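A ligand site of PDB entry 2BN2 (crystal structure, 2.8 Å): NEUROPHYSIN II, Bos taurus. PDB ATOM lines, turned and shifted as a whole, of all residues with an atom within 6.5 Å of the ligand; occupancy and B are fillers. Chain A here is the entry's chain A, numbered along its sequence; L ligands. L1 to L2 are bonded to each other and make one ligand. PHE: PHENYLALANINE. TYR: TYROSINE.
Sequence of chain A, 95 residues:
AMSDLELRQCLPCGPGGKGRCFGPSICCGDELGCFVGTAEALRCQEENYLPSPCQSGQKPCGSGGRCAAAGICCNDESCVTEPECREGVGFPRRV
OH of TYR L2 lies within hydrogen-bond range of O of Gly 23 (3.2 Å).
N of PHE L1 lies within hydrogen-bond range of O of Leu 50 (2.6 Å).
The side-chain carboxylate of Glu 47 is in salt-bridge range of a nitrogen (N) of PHE L1, at 2.8 Å.
A nitrogen (N) of PHE L1 is in hydrogen-bond range of the backbone carbonyl oxygen (O) of Glu 47, 3.0 Å away.
The backbone carbonyl oxygen (O) of Cys 44 sits at hydrogen-bond distance from an oxygen (OH) of TYR L2, 2.6 Å away.
The backbone NH of Cys 54 sits at hydrogen-bond distance from an oxygen (O) of PHE L1.
A nitrogen (N) of PHE L1 lies within hydrogen-bond range of the backbone carbonyl oxygen of Ser 52, 2.6 Å away.
The side-chain sulfur (SG) of Cys 21 lies close to an oxygen (OH) of TYR L2 (3.7 Å).
NH2 of Arg 8 is in salt-bridge range of OE2 of Glu 47, 2.8 Å away.
The guanidinium group (NH2) of Arg 8 sits at hydrogen-bond distance from the backbone carbonyl oxygen (O) of Ser 52 (3.2 Å).
The side-chain sulfur of Cys 44 is disulfide-bonded to the side-chain sulfur of Cys 21 (2.0 Å).
The backbone NH (N) of Gln 55 is in hydrogen-bond range of the backbone carbonyl oxygen (O) of Arg 8 (2.9 Å).
OE1 of Glu 47 is in hydrogen-bond range of N of Leu 11, 2.9 Å away.
O of Leu 11 lies within hydrogen-bond range of N of Cys 21 (3.0 Å).
OG of Ser 56 lies within hydrogen-bond range of O of Cys 21, at 2.9 Å.
O of Pro 24 is in hydrogen-bond range of N of Gln 45, at 3.3 Å.
Residues that only touch the ligand: Asn 48 (3.1 Å), Pro 51 (3.2 Å), Pro 24 (3.3 Å), Pro 53 (3.6 Å), Phe 22 (3.7 Å), Cys 10 (3.8 Å) and Arg 8 (3.8 Å).
Of the 25 residues printed, 14 come within 4 Å of the ligand.
The nearest printed residue that does not touch the ligand is Asp 76 (4.5 Å).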
ATOM      1  N   ARG A   8      -6.872  -8.187 -15.406  1.00  0.00           N
ATOM      2  CA  ARG A   8      -7.559  -7.317 -14.448  1.00  0.00           C
ATOM      3  C   ARG A   8      -7.996  -8.053 -13.184  1.00  0.00           C
ATOM      4  O   ARG A   8      -8.201  -9.269 -13.219  1.00  0.00           O
ATOM      5  CB  ARG A   8      -8.775  -6.644 -15.082  1.00  0.00           C
ATOM      6  CG  ARG A   8      -9.885  -7.599 -15.517  1.00  0.00           C
ATOM      7  CD  ARG A   8     -11.299  -7.026 -15.305  1.00  0.00           C
ATOM      8  NE  ARG A   8     -12.326  -7.884 -15.906  1.00  0.00           N
ATOM      9  CZ  ARG A   8     -13.300  -8.498 -15.250  1.00  0.00           C
ATOM     10  NH1 ARG A   8     -13.441  -8.329 -13.939  1.00  0.00           N
ATOM     11  NH2 ARG A   8     -14.107  -9.345 -15.893  1.00  0.00           N
ATOM     12  N   CYS A  10     -10.902  -8.806 -10.241  1.00  0.00           N
ATOM     13  CA  CYS A  10     -12.333  -9.041 -10.404  1.00  0.00           C
ATOM     14  C   CYS A  10     -13.102  -7.901  -9.784  1.00  0.00           C
ATOM     15  O   CYS A  10     -12.494  -6.995  -9.234  1.00  0.00           O
ATOM     16  CB  CYS A  10     -12.709 -10.360  -9.756  1.00  0.00           C
ATOM     17  SG  CYS A  10     -11.673 -11.726 -10.365  1.00  0.00           S
ATOM     18  N   LEU A  11     -14.428  -7.926  -9.855  1.00  0.00           N
ATOM     19  CA  LEU A  11     -15.222  -6.839  -9.307  1.00  0.00           C
ATOM     20  C   LEU A  11     -14.770  -6.526  -7.881  1.00  0.00           C
ATOM     21  O   LEU A  11     -14.206  -7.387  -7.205  1.00  0.00           O
ATOM     22  CB  LEU A  11     -16.705  -7.185  -9.286  1.00  0.00           C
ATOM     23  CG  LEU A  11     -17.297  -7.521 -10.644  1.00  0.00           C
ATOM     24  CD1 LEU A  11     -18.686  -8.020 -10.460  1.00  0.00           C
ATOM     25  CD2 LEU A  11     -17.283  -6.303 -11.514  1.00  0.00           C
ATOM     26  N   CYS A  21     -13.083  -9.511  -5.492  1.00  0.00           N
ATOM     27  CA  CYS A  21     -13.617 -10.849  -5.564  1.00  0.00           C
ATOM     28  C   CYS A  21     -12.585 -11.870  -5.979  1.00  0.00           C
ATOM     29  O   CYS A  21     -11.981 -11.759  -7.051  1.00  0.00           O
ATOM     30  CB  CYS A  21     -14.791 -10.860  -6.532  1.00  0.00           C
ATOM     31  SG  CYS A  21     -16.182  -9.909  -5.870  1.00  0.00           S
ATOM     32  N   PHE A  22     -12.344 -12.842  -5.104  1.00  0.00           N
ATOM     33  CA  PHE A  22     -11.425 -13.932  -5.427  1.00  0.00           C
ATOM     34  C   PHE A  22     -12.161 -15.136  -5.982  1.00  0.00           C
ATOM     35  O   PHE A  22     -11.585 -15.953  -6.699  1.00  0.00           O
ATOM     36  CB  PHE A  22     -10.611 -14.337  -4.208  1.00  0.00           C
ATOM     37  CG  PHE A  22      -9.560 -13.338  -3.841  1.00  0.00           C
ATOM     38  CD1 PHE A  22      -9.915 -12.043  -3.497  1.00  0.00           C
ATOM     39  CD2 PHE A  22      -8.219 -13.662  -3.950  1.00  0.00           C
ATOM     40  CE1 PHE A  22      -8.960 -11.074  -3.269  1.00  0.00           C
ATOM     41  CE2 PHE A  22      -7.254 -12.699  -3.731  1.00  0.00           C
ATOM     42  CZ  PHE A  22      -7.629 -11.394  -3.391  1.00  0.00           C
ATOM     43  N   GLY A  23     -13.442 -15.219  -5.652  1.00  0.00           N
ATOM     44  CA  GLY A  23     -14.317 -16.205  -6.280  1.00  0.00           C
ATOM     45  C   GLY A  23     -15.761 -15.779  -6.143  1.00  0.00           C
ATOM     46  O   GLY A  23     -16.057 -14.800  -5.444  1.00  0.00           O
ATOM     47  N   PRO A  24     -16.712 -16.540  -6.711  1.00  0.00           N
ATOM     48  CA  PRO A  24     -18.121 -16.155  -6.681  1.00  0.00           C
ATOM     49  C   PRO A  24     -18.664 -15.880  -5.281  1.00  0.00           C
ATOM     50  O   PRO A  24     -19.606 -15.109  -5.130  1.00  0.00           O
ATOM     51  CB  PRO A  24     -18.829 -17.349  -7.336  1.00  0.00           C
ATOM     52  CG  PRO A  24     -17.843 -18.441  -7.360  1.00  0.00           C
ATOM     53  CD  PRO A  24     -16.494 -17.815  -7.408  1.00  0.00           C
ATOM     54  N   SER A  25     -18.013 -16.427  -4.260  1.00  0.00           N
ATOM     55  CA  SER A  25     -18.404 -16.113  -2.880  1.00  0.00           C
ATOM     56  C   SER A  25     -17.263 -15.830  -1.905  1.00  0.00           C
ATOM     57  O   SER A  25     -17.450 -15.894  -0.699  1.00  0.00           O
ATOM     58  CB  SER A  25     -19.290 -17.217  -2.303  1.00  0.00           C
ATOM     59  OG  SER A  25     -18.645 -18.474  -2.339  1.00  0.00           O
ATOM     60  N   ILE A  26     -16.091 -15.484  -2.428  1.00  0.00           N
ATOM     61  CA  ILE A  26     -15.010 -14.986  -1.587  1.00  0.00           C
ATOM     62  C   ILE A  26     -14.739 -13.527  -1.905  1.00  0.00           C
ATOM     63  O   ILE A  26     -14.412 -13.179  -3.030  1.00  0.00           O
ATOM     64  CB  ILE A  26     -13.711 -15.785  -1.799  1.00  0.00           C
ATOM     65  CG1 ILE A  26     -13.908 -17.222  -1.358  1.00  0.00           C
ATOM     66  CG2 ILE A  26     -12.583 -15.175  -0.979  1.00  0.00           C
ATOM     67  CD1 ILE A  26     -13.316 -18.202  -2.294  1.00  0.00           C
ATOM     68  N   ALA A  41     -19.870 -10.901   0.372  1.00  0.00           N
ATOM     69  CA  ALA A  41     -19.287 -11.601  -0.760  1.00  0.00           C
ATOM     70  C   ALA A  41     -20.306 -11.805  -1.868  1.00  0.00           C
ATOM     71  O   ALA A  41     -19.968 -12.290  -2.949  1.00  0.00           O
ATOM     72  CB  ALA A  41     -18.756 -12.924  -0.323  1.00  0.00           C
ATOM     73  N   ARG A  43     -21.968  -9.873  -3.914  1.00  0.00           N
ATOM     74  CA  ARG A  43     -21.631  -9.146  -5.143  1.00  0.00           C
ATOM     75  C   ARG A  43     -20.706  -9.895  -6.093  1.00  0.00           C
ATOM     76  O   ARG A  43     -20.717  -9.644  -7.292  1.00  0.00           O
ATOM     77  CB  ARG A  43     -20.982  -7.807  -4.801  1.00  0.00           C
ATOM     78  CG  ARG A  43     -21.103  -6.765  -5.885  1.00  0.00           C
ATOM     79  CD  ARG A  43     -19.876  -6.680  -6.792  1.00  0.00           C
ATOM     80  NE  ARG A  43     -20.244  -6.155  -8.107  1.00  0.00           N
ATOM     81  CZ  ARG A  43     -19.930  -4.945  -8.550  1.00  0.00           C
ATOM     82  NH1 ARG A  43     -19.039  -4.195  -7.925  1.00  0.00           N
ATOM     83  NH2 ARG A  43     -20.461  -4.521  -9.692  1.00  0.00           N
ATOM     84  N   CYS A  44     -19.876 -10.789  -5.552  1.00  0.00           N
ATOM     85  CA  CYS A  44     -18.897 -11.536  -6.355  1.00  0.00           C
ATOM     86  C   CYS A  44     -19.528 -12.516  -7.313  1.00  0.00           C
ATOM     87  O   CYS A  44     -18.867 -13.006  -8.236  1.00  0.00           O
ATOM     88  CB  CYS A  44     -17.939 -12.274  -5.437  1.00  0.00           C
ATOM     89  SG  CYS A  44     -16.956 -11.133  -4.455  1.00  0.00           S
ATOM     90  N   GLN A  45     -20.803 -12.792  -7.114  1.00  0.00           N
ATOM     91  CA  GLN A  45     -21.546 -13.646  -8.022  1.00  0.00           C
ATOM     92  C   GLN A  45     -21.704 -12.929  -9.368  1.00  0.00           C
ATOM     93  O   GLN A  45     -21.715 -13.549 -10.431  1.00  0.00           O
ATOM     94  CB  GLN A  45     -22.924 -13.948  -7.421  1.00  0.00           C
ATOM     95  CG  GLN A  45     -23.447 -15.360  -7.717  1.00  0.00           C
ATOM     96  CD  GLN A  45     -22.947 -16.402  -6.723  1.00  0.00           C
ATOM     97  OE1 GLN A  45     -22.581 -17.504  -7.112  1.00  0.00           O
ATOM     98  NE2 GLN A  45     -22.998 -16.070  -5.443  1.00  0.00           N
ATOM     99  N   GLU A  46     -21.623 -11.615  -9.314  1.00  0.00           N
ATOM    100  CA  GLU A  46     -21.849 -10.779 -10.481  1.00  0.00           C
ATOM    101  C   GLU A  46     -20.749 -10.924 -11.514  1.00  0.00           C
ATOM    102  O   GLU A  46     -21.004 -10.897 -12.719  1.00  0.00           O
ATOM    103  CB  GLU A  46     -21.952  -9.339 -10.027  1.00  0.00           C
ATOM    104  CG  GLU A  46     -22.912  -8.511 -10.811  1.00  0.00           C
ATOM    105  CD  GLU A  46     -23.435  -7.356 -10.005  1.00  0.00           C
ATOM    106  OE1 GLU A  46     -22.700  -6.363  -9.814  1.00  0.00           O
ATOM    107  OE2 GLU A  46     -24.564  -7.481  -9.497  1.00  0.00           O
ATOM    108  N   GLU A  47     -19.556 -11.265 -11.048  1.00  0.00           N
ATOM    109  CA  GLU A  47     -18.405 -11.457 -11.918  1.00  0.00           C
ATOM    110  C   GLU A  47     -18.604 -12.545 -12.965  1.00  0.00           C
ATOM    111  O   GLU A  47     -17.965 -12.512 -14.028  1.00  0.00           O
ATOM    112  CB  GLU A  47     -17.153 -11.778 -11.097  1.00  0.00           C
ATOM    113  CG  GLU A  47     -15.907 -12.071 -11.913  1.00  0.00           C
ATOM    114  CD  GLU A  47     -15.316 -10.842 -12.580  1.00  0.00           C
ATOM    115  OE1 GLU A  47     -15.069  -9.837 -11.870  1.00  0.00           O
ATOM    116  OE2 GLU A  47     -15.085 -10.880 -13.798  1.00  0.00           O
ATOM    117  N   ASN A  48     -19.428 -13.531 -12.657  1.00  0.00           N
ATOM    118  CA  ASN A  48     -19.657 -14.642 -13.585  1.00  0.00           C
ATOM    119  C   ASN A  48     -20.468 -14.191 -14.785  1.00  0.00           C
ATOM    120  O   ASN A  48     -20.655 -14.950 -15.723  1.00  0.00           O
ATOM    121  CB  ASN A  48     -20.391 -15.779 -12.894  1.00  0.00           C
ATOM    122  CG  ASN A  48     -19.618 -16.343 -11.731  1.00  0.00           C
ATOM    123  OD1 ASN A  48     -18.402 -16.591 -11.819  1.00  0.00           O
ATOM    124  ND2 ASN A  48     -20.307 -16.554 -10.620  1.00  0.00           N
ATOM    125  N   TYR A  49     -21.015 -12.987 -14.712  1.00  0.00           N
ATOM    126  CA  TYR A  49     -21.716 -12.394 -15.838  1.00  0.00           C
ATOM    127  C   TYR A  49     -20.792 -11.672 -16.809  1.00  0.00           C
ATOM    128  O   TYR A  49     -21.155 -11.446 -17.961  1.00  0.00           O
ATOM    129  CB  TYR A  49     -22.777 -11.419 -15.325  1.00  0.00           C
ATOM    130  CG  TYR A  49     -23.885 -12.108 -14.571  1.00  0.00           C
ATOM    131  CD1 TYR A  49     -23.700 -12.519 -13.255  1.00  0.00           C
ATOM    132  CD2 TYR A  49     -25.089 -12.405 -15.198  1.00  0.00           C
ATOM    133  CE1 TYR A  49     -24.689 -13.217 -12.584  1.00  0.00           C
ATOM    134  CE2 TYR A  49     -26.069 -13.109 -14.536  1.00  0.00           C
ATOM    135  CZ  TYR A  49     -25.863 -13.512 -13.225  1.00  0.00           C
ATOM    136  OH  TYR A  49     -26.788 -14.292 -12.592  1.00  0.00           O
ATOM    137  N   LEU A  50     -19.588 -11.314 -16.356  1.00  0.00           N
ATOM    138  CA  LEU A  50     -18.622 -10.613 -17.201  1.00  0.00           C
ATOM    139  C   LEU A  50     -17.807 -11.545 -18.096  1.00  0.00           C
ATOM    140  O   LEU A  50     -17.161 -12.480 -17.601  1.00  0.00           O
ATOM    141  CB  LEU A  50     -17.690  -9.764 -16.346  1.00  0.00           C
ATOM    142  CG  LEU A  50     -18.302  -8.513 -15.741  1.00  0.00           C
ATOM    143  CD1 LEU A  50     -17.249  -7.768 -14.995  1.00  0.00           C
ATOM    144  CD2 LEU A  50     -18.895  -7.632 -16.821  1.00  0.00           C
ATOM    145  N   PRO A  51     -17.705 -11.200 -19.402  1.00  0.00           N
ATOM    146  CA  PRO A  51     -17.273 -12.112 -20.495  1.00  0.00           C
ATOM    147  C   PRO A  51     -15.770 -12.231 -20.616  1.00  0.00           C
ATOM    148  O   PRO A  51     -15.236 -12.835 -21.547  1.00  0.00           O
ATOM    149  CB  PRO A  51     -17.844 -11.473 -21.748  1.00  0.00           C
ATOM    150  CG  PRO A  51     -18.355 -10.137 -21.348  1.00  0.00           C
ATOM    151  CD  PRO A  51     -18.067  -9.882 -19.915  1.00  0.00           C
ATOM    152  N   SER A  52     -15.128 -11.775 -19.564  1.00  0.00           N
ATOM    153  CA  SER A  52     -13.739 -11.358 -19.550  1.00  0.00           C
ATOM    154  C   SER A  52     -13.023 -12.054 -18.341  1.00  0.00           C
ATOM    155  O   SER A  52     -13.586 -12.162 -17.262  1.00  0.00           O
ATOM    156  CB  SER A  52     -13.804  -9.847 -19.370  1.00  0.00           C
ATOM    157  OG  SER A  52     -12.598  -9.265 -18.990  1.00  0.00           O
ATOM    158  N   PRO A  53     -11.813 -12.655 -18.618  1.00  0.00           N
ATOM    159  CA  PRO A  53     -10.987 -13.312 -17.553  1.00  0.00           C
ATOM    160  C   PRO A  53     -10.453 -12.309 -16.546  1.00  0.00           C
ATOM    161  O   PRO A  53      -9.978 -11.264 -16.960  1.00  0.00           O
ATOM    162  CB  PRO A  53      -9.841 -13.940 -18.378  1.00  0.00           C
ATOM    163  CG  PRO A  53     -10.006 -13.502 -19.804  1.00  0.00           C
ATOM    164  CD  PRO A  53     -11.285 -12.725 -19.927  1.00  0.00           C
ATOM    165  N   CYS A  54     -10.716 -12.498 -15.263  1.00  0.00           N
ATOM    166  CA  CYS A  54     -10.055 -11.760 -14.143  1.00  0.00           C
ATOM    167  C   CYS A  54      -9.278 -12.682 -13.178  1.00  0.00           C
ATOM    168  O   CYS A  54      -9.422 -13.896 -13.205  1.00  0.00           O
ATOM    169  CB  CYS A  54     -11.071 -10.963 -13.297  1.00  0.00           C
ATOM    170  SG  CYS A  54     -12.232 -11.971 -12.298  1.00  0.00           S
ATOM    171  N   GLN A  55      -8.383 -12.092 -12.391  1.00  0.00           N
ATOM    172  CA  GLN A  55      -7.681 -12.797 -11.338  1.00  0.00           C
ATOM    173  C   GLN A  55      -7.303 -11.747 -10.303  1.00  0.00           C
ATOM    174  O   GLN A  55      -6.729 -10.731 -10.660  1.00  0.00           O
ATOM    175  CB  GLN A  55      -6.431 -13.467 -11.889  1.00  0.00           C
ATOM    176  CG  GLN A  55      -5.477 -13.999 -10.836  1.00  0.00           C
ATOM    177  CD  GLN A  55      -6.140 -15.023  -9.925  1.00  0.00           C
ATOM    178  OE1 GLN A  55      -6.388 -16.158 -10.340  1.00  0.00           O
ATOM    179  NE2 GLN A  55      -6.519 -14.604  -8.722  1.00  0.00           N
ATOM    180  N   SER A  56      -7.805 -11.881  -9.084  1.00  0.00           N
ATOM    181  CA  SER A  56      -7.482 -10.887  -8.071  1.00  0.00           C
ATOM    182  C   SER A  56      -6.188 -11.275  -7.399  1.00  0.00           C
ATOM    183  O   SER A  56      -5.748 -12.416  -7.491  1.00  0.00           O
ATOM    184  CB  SER A  56      -8.604 -10.772  -7.031  1.00  0.00           C
ATOM    185  OG  SER A  56      -9.704 -10.044  -7.541  1.00  0.00           O
ATOM    186  N   ASP A  76     -10.560 -19.703  -5.853  1.00  0.00           N
ATOM    187  CA  ASP A  76     -11.944 -19.307  -6.061  1.00  0.00           C
ATOM    188  C   ASP A  76     -12.966 -20.209  -5.386  1.00  0.00           C
ATOM    189  O   ASP A  76     -14.173 -20.052  -5.593  1.00  0.00           O
ATOM    190  CB  ASP A  76     -12.241 -19.184  -7.563  1.00  0.00           C
ATOM    191  CG  ASP A  76     -12.106 -20.501  -8.299  1.00  0.00           C
ATOM    192  OD1 ASP A  76     -11.247 -21.341  -7.942  1.00  0.00           O
ATOM    193  OD2 ASP A  76     -12.840 -20.666  -9.296  1.00  0.00           O
HETATM  194  N   PHE L   1     -15.469 -12.894 -15.652  1.00  0.00           N
HETATM  195  CA  PHE L   1     -15.594 -14.221 -14.978  1.00  0.00           C
HETATM  196  C   PHE L   1     -14.283 -14.656 -14.326  1.00  0.00           C
HETATM  197  O   PHE L   1     -13.212 -14.197 -14.723  1.00  0.00           O
HETATM  198  CB  PHE L   1     -16.031 -15.284 -15.980  1.00  0.00           C
HETATM  199  CG  PHE L   1     -15.067 -15.498 -17.103  1.00  0.00           C
HETATM  200  CD1 PHE L   1     -13.950 -16.312 -16.937  1.00  0.00           C
HETATM  201  CD2 PHE L   1     -15.279 -14.893 -18.346  1.00  0.00           C
HETATM  202  CE1 PHE L   1     -13.064 -16.521 -17.978  1.00  0.00           C
HETATM  203  CE2 PHE L   1     -14.393 -15.102 -19.387  1.00  0.00           C
HETATM  204  CZ  PHE L   1     -13.276 -15.919 -19.208  1.00  0.00           C
HETATM  205  N   TYR L   2     -14.376 -15.558 -13.356  1.00  0.00           N
HETATM  206  CA  TYR L   2     -13.217 -16.050 -12.616  1.00  0.00           C
HETATM  207  C   TYR L   2     -12.298 -16.977 -13.415  1.00  0.00           C
HETATM  208  O   TYR L   2     -12.723 -18.037 -13.876  1.00  0.00           O
HETATM  209  CB  TYR L   2     -13.681 -16.752 -11.336  1.00  0.00           C
HETATM  210  CG  TYR L   2     -14.386 -15.837 -10.380  1.00  0.00           C
HETATM  211  CD1 TYR L   2     -13.654 -14.949  -9.595  1.00  0.00           C
HETATM  212  CD2 TYR L   2     -15.774 -15.762 -10.344  1.00  0.00           C
HETATM  213  CE1 TYR L   2     -14.281 -14.009  -8.808  1.00  0.00           C
HETATM  214  CE2 TYR L   2     -16.420 -14.815  -9.549  1.00  0.00           C
HETATM  215  CZ  TYR L   2     -15.659 -13.944  -8.790  1.00  0.00           C
HETATM  216  OH  TYR L   2     -16.234 -12.948  -8.062  1.00  0.00           O
